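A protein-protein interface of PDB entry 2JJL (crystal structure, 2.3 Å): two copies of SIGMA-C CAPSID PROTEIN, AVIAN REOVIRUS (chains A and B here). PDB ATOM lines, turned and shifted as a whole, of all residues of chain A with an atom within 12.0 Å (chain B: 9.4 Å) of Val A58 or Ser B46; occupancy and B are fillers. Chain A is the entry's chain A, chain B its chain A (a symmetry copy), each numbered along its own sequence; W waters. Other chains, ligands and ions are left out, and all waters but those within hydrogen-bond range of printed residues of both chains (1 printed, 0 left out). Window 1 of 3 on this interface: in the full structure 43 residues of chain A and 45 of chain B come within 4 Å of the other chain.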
ATOM      1  N   SER A  42     -26.605  -5.334   1.718  1.00  0.00           N
ATOM      2  CA  SER A  42     -25.333  -5.479   2.440  1.00  0.00           C
ATOM      3  C   SER A  42     -24.451  -6.667   2.008  1.00  0.00           C
ATOM      4  O   SER A  42     -23.277  -6.723   2.380  1.00  0.00           O
ATOM      5  CB  SER A  42     -25.567  -5.493   3.960  1.00  0.00           C
ATOM      6  OG  SER A  42     -25.645  -6.809   4.484  1.00  0.00           O
ATOM      7  N   GLY A  44     -22.123  -8.553  -0.570  1.00  0.00           N
ATOM      8  CA  GLY A  44     -21.223  -7.970  -1.582  1.00  0.00           C
ATOM      9  C   GLY A  44     -20.962  -6.457  -1.481  1.00  0.00           C
ATOM     10  O   GLY A  44     -20.884  -5.755  -2.500  1.00  0.00           O
ATOM     11  N   LEU A  45     -20.867  -5.951  -0.248  1.00  0.00           N
ATOM     12  CA  LEU A  45     -20.272  -4.646   0.021  1.00  0.00           C
ATOM     13  C   LEU A  45     -18.767  -4.779  -0.245  1.00  0.00           C
ATOM     14  O   LEU A  45     -18.134  -5.765   0.175  1.00  0.00           O
ATOM     15  CB  LEU A  45     -20.483  -4.243   1.481  1.00  0.00           C
ATOM     16  CG  LEU A  45     -21.771  -3.616   2.015  1.00  0.00           C
ATOM     17  CD1 LEU A  45     -21.729  -3.566   3.551  1.00  0.00           C
ATOM     18  CD2 LEU A  45     -22.026  -2.233   1.447  1.00  0.00           C
ATOM     19  N   SER A  46     -18.196  -3.812  -0.962  1.00  0.00           N
ATOM     20  CA  SER A  46     -16.734  -3.722  -1.058  1.00  0.00           C
ATOM     21  C   SER A  46     -16.223  -2.347  -0.597  1.00  0.00           C
ATOM     22  O   SER A  46     -16.997  -1.414  -0.394  1.00  0.00           O
ATOM     23  CB  SER A  46     -16.221  -4.083  -2.458  1.00  0.00           C
ATOM     24  OG  SER A  46     -16.796  -3.249  -3.439  1.00  0.00           O
ATOM     25  N   PHE A  47     -14.907  -2.247  -0.444  1.00  0.00           N
ATOM     26  CA  PHE A  47     -14.272  -1.124   0.218  1.00  0.00           C
ATOM     27  C   PHE A  47     -13.107  -0.647  -0.627  1.00  0.00           C
ATOM     28  O   PHE A  47     -12.146  -1.397  -0.852  1.00  0.00           O
ATOM     29  CB  PHE A  47     -13.823  -1.546   1.627  1.00  0.00           C
ATOM     30  CG  PHE A  47     -14.977  -1.927   2.535  1.00  0.00           C
ATOM     31  CD1 PHE A  47     -15.623  -0.966   3.302  1.00  0.00           C
ATOM     32  CD2 PHE A  47     -15.435  -3.251   2.595  1.00  0.00           C
ATOM     33  CE1 PHE A  47     -16.695  -1.313   4.133  1.00  0.00           C
ATOM     34  CE2 PHE A  47     -16.505  -3.609   3.418  1.00  0.00           C
ATOM     35  CZ  PHE A  47     -17.138  -2.642   4.187  1.00  0.00           C
ATOM     36  N   SER A  48     -13.222   0.593  -1.112  1.00  0.00           N
ATOM     37  CA  SER A  48     -12.182   1.220  -1.927  1.00  0.00           C
ATOM     38  C   SER A  48     -11.140   1.957  -1.057  1.00  0.00           C
ATOM     39  O   SER A  48     -11.481   2.489   0.002  1.00  0.00           O
ATOM     40  CB  SER A  48     -12.808   2.164  -2.954  1.00  0.00           C
ATOM     41  OG  SER A  48     -13.811   2.963  -2.350  1.00  0.00           O
ATOM     42  N   PRO A  49      -9.863   1.979  -1.495  1.00  0.00           N
ATOM     43  CA  PRO A  49      -8.792   2.698  -0.748  1.00  0.00           C
ATOM     44  C   PRO A  49      -9.146   4.172  -0.430  1.00  0.00           C
ATOM     45  O   PRO A  49      -9.801   4.836  -1.243  1.00  0.00           O
ATOM     46  CB  PRO A  49      -7.588   2.598  -1.686  1.00  0.00           C
ATOM     47  CG  PRO A  49      -7.850   1.314  -2.474  1.00  0.00           C
ATOM     48  CD  PRO A  49      -9.339   1.336  -2.718  1.00  0.00           C
ATOM     49  N   PRO A  50      -8.767   4.673   0.763  1.00  0.00           N
ATOM     50  CA  PRO A  50      -7.926   4.100   1.827  1.00  0.00           C
ATOM     51  C   PRO A  50      -8.605   3.106   2.788  1.00  0.00           C
ATOM     52  O   PRO A  50      -8.014   2.747   3.812  1.00  0.00           O
ATOM     53  CB  PRO A  50      -7.501   5.342   2.607  1.00  0.00           C
ATOM     54  CG  PRO A  50      -8.725   6.222   2.528  1.00  0.00           C
ATOM     55  CD  PRO A  50      -9.265   6.015   1.132  1.00  0.00           C
ATOM     56  N   LEU A  51      -9.832   2.690   2.485  1.00  0.00           N
ATOM     57  CA  LEU A  51     -10.503   1.621   3.258  1.00  0.00           C
ATOM     58  C   LEU A  51     -10.095   0.262   2.709  1.00  0.00           C
ATOM     59  O   LEU A  51      -9.925   0.109   1.504  1.00  0.00           O
ATOM     60  CB  LEU A  51     -12.019   1.751   3.196  1.00  0.00           C
ATOM     61  CG  LEU A  51     -12.604   3.054   3.717  1.00  0.00           C
ATOM     62  CD1 LEU A  51     -14.086   3.114   3.410  1.00  0.00           C
ATOM     63  CD2 LEU A  51     -12.348   3.215   5.215  1.00  0.00           C
ATOM     64  N   SER A  52      -9.910  -0.714   3.590  1.00  0.00           N
ATOM     65  CA  SER A  52      -9.578  -2.059   3.145  1.00  0.00           C
ATOM     66  C   SER A  52     -10.126  -3.142   4.078  1.00  0.00           C
ATOM     67  O   SER A  52     -10.449  -2.866   5.245  1.00  0.00           O
ATOM     68  CB  SER A  52      -8.064  -2.207   2.933  1.00  0.00           C
ATOM     69  OG  SER A  52      -7.382  -2.322   4.164  1.00  0.00           O
ATOM     70  N   VAL A  53     -10.247  -4.362   3.544  1.00  0.00           N
ATOM     71  CA  VAL A  53     -10.701  -5.549   4.308  1.00  0.00           C
ATOM     72  C   VAL A  53      -9.630  -6.644   4.320  1.00  0.00           C
ATOM     73  O   VAL A  53      -9.016  -6.949   3.291  1.00  0.00           O
ATOM     74  CB  VAL A  53     -12.004  -6.183   3.737  1.00  0.00           C
ATOM     75  CG1 VAL A  53     -12.751  -6.961   4.832  1.00  0.00           C
ATOM     76  CG2 VAL A  53     -12.903  -5.142   3.149  1.00  0.00           C
ATOM     77  N   ALA A  54      -9.415  -7.231   5.491  1.00  0.00           N
ATOM     78  CA  ALA A  54      -8.548  -8.395   5.627  1.00  0.00           C
ATOM     79  C   ALA A  54      -9.148  -9.277   6.707  1.00  0.00           C
ATOM     80  O   ALA A  54      -9.356  -8.821   7.845  1.00  0.00           O
ATOM     81  CB  ALA A  54      -7.110  -7.987   5.987  1.00  0.00           C
ATOM     82  N   ASP A  55      -9.453 -10.525   6.329  1.00  0.00           N
ATOM     83  CA  ASP A  55     -10.067 -11.525   7.227  1.00  0.00           C
ATOM     84  C   ASP A  55     -11.303 -10.989   7.938  1.00  0.00           C
ATOM     85  O   ASP A  55     -11.415 -11.094   9.166  1.00  0.00           O
ATOM     86  CB  ASP A  55      -9.048 -12.043   8.263  1.00  0.00           C
ATOM     87  CG  ASP A  55      -7.676 -12.334   7.653  1.00  0.00           C
ATOM     88  OD1 ASP A  55      -7.608 -12.895   6.528  1.00  0.00           O
ATOM     89  OD2 ASP A  55      -6.661 -11.995   8.306  1.00  0.00           O
ATOM     90  N   GLY A  56     -12.212 -10.391   7.168  1.00  0.00           N
ATOM     91  CA  GLY A  56     -13.431  -9.782   7.723  1.00  0.00           C
ATOM     92  C   GLY A  56     -13.320  -8.432   8.440  1.00  0.00           C
ATOM     93  O   GLY A  56     -14.348  -7.811   8.747  1.00  0.00           O
ATOM     94  N   VAL A  57     -12.094  -7.977   8.723  1.00  0.00           N
ATOM     95  CA  VAL A  57     -11.877  -6.692   9.426  1.00  0.00           C
ATOM     96  C   VAL A  57     -11.756  -5.540   8.414  1.00  0.00           C
ATOM     97  O   VAL A  57     -10.945  -5.594   7.500  1.00  0.00           O
ATOM     98  CB  VAL A  57     -10.650  -6.744  10.380  1.00  0.00           C
ATOM     99  CG1 VAL A  57     -10.600  -5.503  11.282  1.00  0.00           C
ATOM    100  CG2 VAL A  57     -10.713  -7.987  11.265  1.00  0.00           C
ATOM    101  N   VAL A  58     -12.609  -4.530   8.546  1.00  0.00           N
ATOM    102  CA  VAL A  58     -12.476  -3.316   7.745  1.00  0.00           C
ATOM    103  C   VAL A  58     -11.604  -2.305   8.508  1.00  0.00           C
ATOM    104  O   VAL A  58     -11.832  -2.042   9.698  1.00  0.00           O
ATOM    105  CB  VAL A  58     -13.849  -2.701   7.367  1.00  0.00           C
ATOM    106  CG1 VAL A  58     -13.662  -1.437   6.482  1.00  0.00           C
ATOM    107  CG2 VAL A  58     -14.724  -3.745   6.641  1.00  0.00           C
ATOM    108  N   SER A  59     -10.587  -1.790   7.814  1.00  0.00           N
ATOM    109  CA  SER A  59      -9.603  -0.868   8.366  1.00  0.00           C
ATOM    110  C   SER A  59      -9.548   0.400   7.541  1.00  0.00           C
ATOM    111  O   SER A  59      -9.799   0.371   6.325  1.00  0.00           O
ATOM    112  CB  SER A  59      -8.205  -1.494   8.336  1.00  0.00           C
ATOM    113  OG  SER A  59      -7.994  -2.364   9.427  1.00  0.00           O
ATOM    114  N   LEU A  60      -9.229   1.518   8.203  1.00  0.00           N
ATOM    115  CA  LEU A  60      -8.706   2.700   7.487  1.00  0.00           C
ATOM    116  C   LEU A  60      -7.199   2.585   7.411  1.00  0.00           C
ATOM    117  O   LEU A  60      -6.530   2.569   8.445  1.00  0.00           O
ATOM    118  CB  LEU A  60      -9.095   4.011   8.181  1.00  0.00           C
ATOM    119  CG  LEU A  60      -8.572   5.276   7.488  1.00  0.00           C
ATOM    120  CD1 LEU A  60      -9.266   5.470   6.138  1.00  0.00           C
ATOM    121  CD2 LEU A  60      -8.714   6.515   8.389  1.00  0.00           C
ATOM    122  N   ASP A  61      -6.656   2.472   6.200  1.00  0.00           N
ATOM    123  CA  ASP A  61      -5.203   2.497   6.044  1.00  0.00           C
ATOM    124  C   ASP A  61      -4.659   3.952   6.189  1.00  0.00           C
ATOM    125  O   ASP A  61      -5.077   4.864   5.449  1.00  0.00           O
ATOM    126  CB  ASP A  61      -4.788   1.899   4.696  1.00  0.00           C
ATOM    127  CG  ASP A  61      -5.169   0.421   4.556  1.00  0.00           C
ATOM    128  OD1 ASP A  61      -4.901  -0.363   5.491  1.00  0.00           O
ATOM    129  OD2 ASP A  61      -5.733   0.050   3.500  1.00  0.00           O
ATOM    130  N   MET A  62      -3.718   4.136   7.119  1.00  0.00           N
ATOM    131  CA  MET A  62      -3.212   5.468   7.503  1.00  0.00           C
ATOM    132  C   MET A  62      -1.717   5.646   7.226  1.00  0.00           C
ATOM    133  O   MET A  62      -0.903   4.821   7.655  1.00  0.00           O
ATOM    134  CB  MET A  62      -3.518   5.732   8.969  1.00  0.00           C
ATOM    135  CG  MET A  62      -5.011   5.881   9.238  1.00  0.00           C
ATOM    136  SD  MET A  62      -5.389   5.746  10.992  1.00  0.00           S
ATOM    137  CE  MET A  62      -4.743   4.108  11.392  1.00  0.00           C
ATOM    138  N   GLN A  69      -4.371   6.720  14.638  1.00  0.00           N
ATOM    139  CA  GLN A  69      -5.574   6.673  15.482  1.00  0.00           C
ATOM    140  C   GLN A  69      -5.223   6.576  16.946  1.00  0.00           C
ATOM    141  O   GLN A  69      -4.294   5.868  17.330  1.00  0.00           O
ATOM    142  CB  GLN A  69      -6.573   5.565  15.069  1.00  0.00           C
ATOM    143  CG  GLN A  69      -6.092   4.122  15.214  1.00  0.00           C
ATOM    144  CD  GLN A  69      -6.174   3.565  16.652  1.00  0.00           C
ATOM    145  OE1 GLN A  69      -6.982   3.992  17.488  1.00  0.00           O
ATOM    146  NE2 GLN A  69      -5.322   2.607  16.930  1.00  0.00           N
ATOM    147  N   VAL A  71      -8.099   6.027  19.156  1.00  0.00           N
ATOM    148  CA  VAL A  71      -9.543   5.868  18.981  1.00  0.00           C
ATOM    149  C   VAL A  71     -10.021   6.647  17.755  1.00  0.00           C
ATOM    150  O   VAL A  71     -10.477   6.041  16.777  1.00  0.00           O
ATOM    151  CB  VAL A  71     -10.388   6.184  20.255  1.00  0.00           C
ATOM    152  CG1 VAL A  71     -11.853   5.802  20.033  1.00  0.00           C
ATOM    153  CG2 VAL A  71      -9.817   5.459  21.481  1.00  0.00           C
ATOM    154  N   ALA B  41     -19.617 -13.804   2.763  1.00  0.00           N
ATOM    155  CA  ALA B  41     -18.473 -13.068   3.342  1.00  0.00           C
ATOM    156  C   ALA B  41     -18.848 -11.810   4.150  1.00  0.00           C
ATOM    157  O   ALA B  41     -18.319 -11.598   5.238  1.00  0.00           O
ATOM    158  CB  ALA B  41     -17.440 -12.738   2.258  1.00  0.00           C
ATOM    159  N   SER B  42     -19.784 -11.009   3.637  1.00  0.00           N
ATOM    160  CA  SER B  42     -20.225  -9.783   4.315  1.00  0.00           C
ATOM    161  C   SER B  42     -20.862  -9.981   5.706  1.00  0.00           C
ATOM    162  O   SER B  42     -21.032  -9.009   6.444  1.00  0.00           O
ATOM    163  CB  SER B  42     -21.145  -8.953   3.404  1.00  0.00           C
ATOM    164  OG  SER B  42     -22.519  -9.201   3.653  1.00  0.00           O
ATOM    165  N   HIS B  43     -21.228 -11.218   6.056  1.00  0.00           N
ATOM    166  CA  HIS B  43     -21.727 -11.540   7.405  1.00  0.00           C
ATOM    167  C   HIS B  43     -20.525 -11.499   8.350  1.00  0.00           C
ATOM    168  O   HIS B  43     -19.444 -11.970   7.991  1.00  0.00           O
ATOM    169  CB  HIS B  43     -22.417 -12.930   7.462  1.00  0.00           C
ATOM    170  CG  HIS B  43     -23.754 -12.999   6.762  1.00  0.00           C
ATOM    171  ND1 HIS B  43     -23.976 -13.802   5.665  1.00  0.00           N
ATOM    172  CD2 HIS B  43     -24.940 -12.386   7.018  1.00  0.00           C
ATOM    173  CE1 HIS B  43     -25.232 -13.673   5.265  1.00  0.00           C
ATOM    174  NE2 HIS B  43     -25.842 -12.808   6.061  1.00  0.00           N
ATOM    175  N   GLY B  44     -20.691 -10.926   9.541  1.00  0.00           N
ATOM    176  CA  GLY B  44     -19.557 -10.765  10.470  1.00  0.00           C
ATOM    177  C   GLY B  44     -18.376  -9.914   9.973  1.00  0.00           C
ATOM    178  O   GLY B  44     -17.206 -10.238  10.228  1.00  0.00           O
ATOM    179  N   LEU B  45     -18.682  -8.848   9.229  1.00  0.00           N
ATOM    180  CA  LEU B  45     -17.740  -7.758   8.994  1.00  0.00           C
ATOM    181  C   LEU B  45     -17.574  -7.017  10.328  1.00  0.00           C
ATOM    182  O   LEU B  45     -18.566  -6.742  11.027  1.00  0.00           O
ATOM    183  CB  LEU B  45     -18.287  -6.783   7.951  1.00  0.00           C
ATOM    184  CG  LEU B  45     -18.194  -7.009   6.441  1.00  0.00           C
ATOM    185  CD1 LEU B  45     -19.050  -5.965   5.705  1.00  0.00           C
ATOM    186  CD2 LEU B  45     -16.766  -6.976   5.933  1.00  0.00           C
ATOM    187  N   SER B  46     -16.330  -6.721  10.699  1.00  0.00           N
ATOM    188  CA  SER B  46     -16.086  -5.806  11.821  1.00  0.00           C
ATOM    189  C   SER B  46     -15.207  -4.617  11.399  1.00  0.00           C
ATOM    190  O   SER B  46     -14.634  -4.603  10.312  1.00  0.00           O
ATOM    191  CB  SER B  46     -15.517  -6.531  13.047  1.00  0.00           C
ATOM    192  OG  SER B  46     -14.315  -7.196  12.731  1.00  0.00           O
ATOM    193  N   PHE B  47     -15.112  -3.632  12.284  1.00  0.00           N
ATOM    194  CA  PHE B  47     -14.545  -2.336  11.967  1.00  0.00           C
ATOM    195  C   PHE B  47     -13.575  -1.941  13.062  1.00  0.00           C
ATOM    196  O   PHE B  47     -13.972  -1.775  14.225  1.00  0.00           O
ATOM    197  CB  PHE B  47     -15.675  -1.307  11.804  1.00  0.00           C
ATOM    198  CG  PHE B  47     -16.604  -1.616  10.646  1.00  0.00           C
ATOM    199  CD1 PHE B  47     -16.329  -1.141   9.370  1.00  0.00           C
ATOM    200  CD2 PHE B  47     -17.744  -2.411  10.832  1.00  0.00           C
ATOM    201  CE1 PHE B  47     -17.180  -1.433   8.296  1.00  0.00           C
ATOM    202  CE2 PHE B  47     -18.599  -2.711   9.770  1.00  0.00           C
ATOM    203  CZ  PHE B  47     -18.319  -2.225   8.500  1.00  0.00           C
ATOM    204  N   SER B  48     -12.299  -1.822  12.681  1.00  0.00           N
ATOM    205  CA  SER B  48     -11.234  -1.426  13.603  1.00  0.00           C
ATOM    206  C   SER B  48     -11.068   0.108  13.658  1.00  0.00           C
ATOM    207  O   SER B  48     -11.285   0.792  12.656  1.00  0.00           O
ATOM    208  CB  SER B  48      -9.920  -2.109  13.221  1.00  0.00           C
ATOM    209  OG  SER B  48      -9.707  -2.037  11.822  1.00  0.00           O
ATOM    210  N   PRO B  49     -10.693   0.654  14.835  1.00  0.00           N
ATOM    211  CA  PRO B  49     -10.467   2.120  14.981  1.00  0.00           C
ATOM    212  C   PRO B  49      -9.492   2.700  13.927  1.00  0.00           C
ATOM    213  O   PRO B  49      -8.532   2.024  13.540  1.00  0.00           O
ATOM    214  CB  PRO B  49      -9.903   2.244  16.397  1.00  0.00           C
ATOM    215  CG  PRO B  49     -10.498   1.042  17.130  1.00  0.00           C
ATOM    216  CD  PRO B  49     -10.455  -0.065  16.105  1.00  0.00           C
ATOM    217  N   PRO B  50      -9.756   3.922  13.422  1.00  0.00           N
ATOM    218  CA  PRO B  50     -10.776   4.919  13.789  1.00  0.00           C
ATOM    219  C   PRO B  50     -12.194   4.699  13.229  1.00  0.00           C
ATOM    220  O   PRO B  50     -13.037   5.596  13.334  1.00  0.00           O
ATOM    221  CB  PRO B  50     -10.198   6.204  13.203  1.00  0.00           C
ATOM    222  CG  PRO B  50      -9.538   5.726  11.933  1.00  0.00           C
ATOM    223  CD  PRO B  50      -8.929   4.389  12.289  1.00  0.00           C
ATOM    224  N   LEU B  51     -12.449   3.544  12.619  1.00  0.00           N
ATOM    225  CA  LEU B  51     -13.816   3.178  12.188  1.00  0.00           C
ATOM    226  C   LEU B  51     -14.559   2.529  13.346  1.00  0.00           C
ATOM    227  O   LEU B  51     -13.964   1.795  14.128  1.00  0.00           O
ATOM    228  CB  LEU B  51     -13.793   2.216  11.008  1.00  0.00           C
ATOM    229  CG  LEU B  51     -13.093   2.709   9.751  1.00  0.00           C
ATOM    230  CD1 LEU B  51     -12.981   1.583   8.746  1.00  0.00           C
ATOM    231  CD2 LEU B  51     -13.820   3.911   9.149  1.00  0.00           C
ATOM    232  N   SER B  52     -15.848   2.821  13.475  1.00  0.00           N
ATOM    233  CA  SER B  52     -16.646   2.196  14.520  1.00  0.00           C
ATOM    234  C   SER B  52     -18.110   2.007  14.111  1.00  0.00           C
ATOM    235  O   SER B  52     -18.596   2.668  13.179  1.00  0.00           O
ATOM    236  CB  SER B  52     -16.523   2.972  15.840  1.00  0.00           C
ATOM    237  OG  SER B  52     -17.283   4.162  15.810  1.00  0.00           O
ATOM    238  N   VAL B  53     -18.790   1.085  14.800  1.00  0.00           N
ATOM    239  CA  VAL B  53     -20.231   0.803  14.588  1.00  0.00           C
ATOM    240  C   VAL B  53     -21.038   1.052  15.867  1.00  0.00           C
ATOM    241  O   VAL B  53     -20.632   0.656  16.966  1.00  0.00           O
ATOM    242  CB  VAL B  53     -20.509  -0.663  14.144  1.00  0.00           C
ATOM    243  CG1 VAL B  53     -21.837  -0.751  13.375  1.00  0.00           C
ATOM    244  CG2 VAL B  53     -19.396  -1.197  13.301  1.00  0.00           C
ATOM    245  N   VAL B  58     -22.040   2.741  10.637  1.00  0.00           N
ATOM    246  CA  VAL B  58     -20.582   2.802  10.610  1.00  0.00           C
ATOM    247  C   VAL B  58     -20.144   4.271  10.471  1.00  0.00           C
ATOM    248  O   VAL B  58     -20.647   5.002   9.606  1.00  0.00           O
ATOM    249  CB  VAL B  58     -19.971   1.926   9.485  1.00  0.00           C
ATOM    250  CG1 VAL B  58     -18.419   1.989   9.518  1.00  0.00           C
ATOM    251  CG2 VAL B  58     -20.456   0.466   9.617  1.00  0.00           C
ATOM    252  N   SER B  59     -19.243   4.684  11.365  1.00  0.00           N
ATOM    253  CA  SER B  59     -18.745   6.051  11.451  1.00  0.00           C
ATOM    254  C   SER B  59     -17.234   6.069  11.354  1.00  0.00           C
ATOM    255  O   SER B  59     -16.565   5.108  11.765  1.00  0.00           O
ATOM    256  CB  SER B  59     -19.123   6.674  12.799  1.00  0.00           C
ATOM    257  OG  SER B  59     -20.447   7.162  12.801  1.00  0.00           O
HETATM  258  O   HOH W   1      -8.729   1.133  11.012  1.00  0.00           O
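Val A58 touches Leu B45, but with the chains exchanged Leu A45 does not touch Val B58 (7.4 Å).
Val A58 touches Leu B51, but with the chains exchanged Leu A51 does not touch Val B58 (7.5 Å).
Ser A59 touches Ser B48, but with the chains exchanged Ser A48 does not touch Ser B59 (13.1 Å).
Ser A59 touches Leu B51, but with the chains exchanged Leu A51 does not touch Ser B59 (8.0 Å).
13 positions are printed for both chains.
Of the 19 pairs that touch across the chains among the printed residues, 2 have their exchanged pair printed and touching as well.
The backbone carbonyl oxygen (O) of Ser A52 sits at hydrogen-bond distance from the backbone NH (N) of Ser A59 (2.8 Å).
The side-chain amide oxygen (OE1) of Gln A69 is in hydrogen-bond range of the backbone NH (N) of Val A71, at 2.9 Å.
The backbone carbonyl oxygen (O) of Ser A42 is in hydrogen-bond range of the side-chain hydroxyl (OG) of Ser B42, 2.9 Å away.
The backbone NH of Ser B46 sits at hydrogen-bond distance from the backbone carbonyl oxygen of Gly A56, 3.0 Å away.
The backbone carbonyl oxygen (O) of Ser B46 is in hydrogen-bond range of the backbone NH (N) of Val A58, 2.7 Å away.
The backbone carbonyl oxygen (O) of Val A58 lies within hydrogen-bond range of the side-chain hydroxyl (OG) of Ser B48.
OG of Ser A59 is in hydrogen-bond range of OG of Ser B48.
Water W1 lies within hydrogen-bond range of O of Pro B49 (2.7 Å), N of Leu A60 (2.9 Å) and O of Ser B48 (3.1 Å).
Of the 22 printed residues of chain A, 9 touch a printed residue of chain B.
Of the 15 printed residues of chain B, 8 touch a printed residue of chain A.
Among the printed residues, no Asp or Glu carboxylate lies within 4 Å of a Lys or Arg side-chain nitrogen of the other chain.
Val A58 touches just these residues of chain B: Leu B45, Ser B46, Phe B47, Ser B48 and Leu B51.
Ser B46 touches just these residues of chain A: Gly A56 (3.0 Å), Val A57 (3.6 Å) and Val A58 (2.7 Å).
Val A57 touches two residues of chain B.
Of the printed residues of chain B, Ser A59 touches Ser B48 and Leu B51.
No residue of chain A comes within 4 Å of Gly B44.
Of chain A, only Gly A56 and Val A58 come within 4 Å of Leu B45.
Of the printed residues of chain A, Phe B47 touches Val A58.
Ser B48 touches three residues of chain A.
Leu B51 touches just these residues of chain A: Leu A51, Val A58, Ser A59 and Leu A60.
Of the printed residues of chain B, Leu A60 touches Pro B50 and Leu B51.
Of the printed residues of chain B, Val A71 touches Pro B49 (3.9 Å) and Pro B50 (3.2 Å).
Of the printed residues of chain B, Leu A51 touches Leu B51 (3.9 Å).
Gly A44 touches none of the printed residues of chain B.
Val A53 touches none of the printed residues of chain B.
The nearest residue of chain B that does not touch Val A58 is Pro B49 (5.9 Å).
The nearest residue of chain A that does not touch Ser B46 is Ser A59 (5.5 Å).
The nearest printed residue of chain A that does not touch Pro B49 is Met A62 (4.8 Å).
Among the printed residues, pairs that only touch across the chains: Val A71 with Pro B50 (3.2 Å), Gly A56 with Leu B45 (3.4 Å), Val A58 with Phe B47 (3.5 Å), Val A57 with Ser B46 (3.6 Å), Gln A69 with Pro B49 (3.6 Å), Val A57 with Ser B48 (3.6 Å), Leu A60 with Pro B50 (3.7 Å), Leu A60 with Leu B51 (3.8 Å), Ser A59 with Leu B51 (3.8 Å), Gln A69 with Pro B50 (3.8 Å), Val A58 with Leu B51 (3.8 Å), Val A71 with Pro B49 (3.9 Å), Val A58 with Leu B45 (3.9 Å) and Leu A51 with Leu B51 (3.9 Å).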
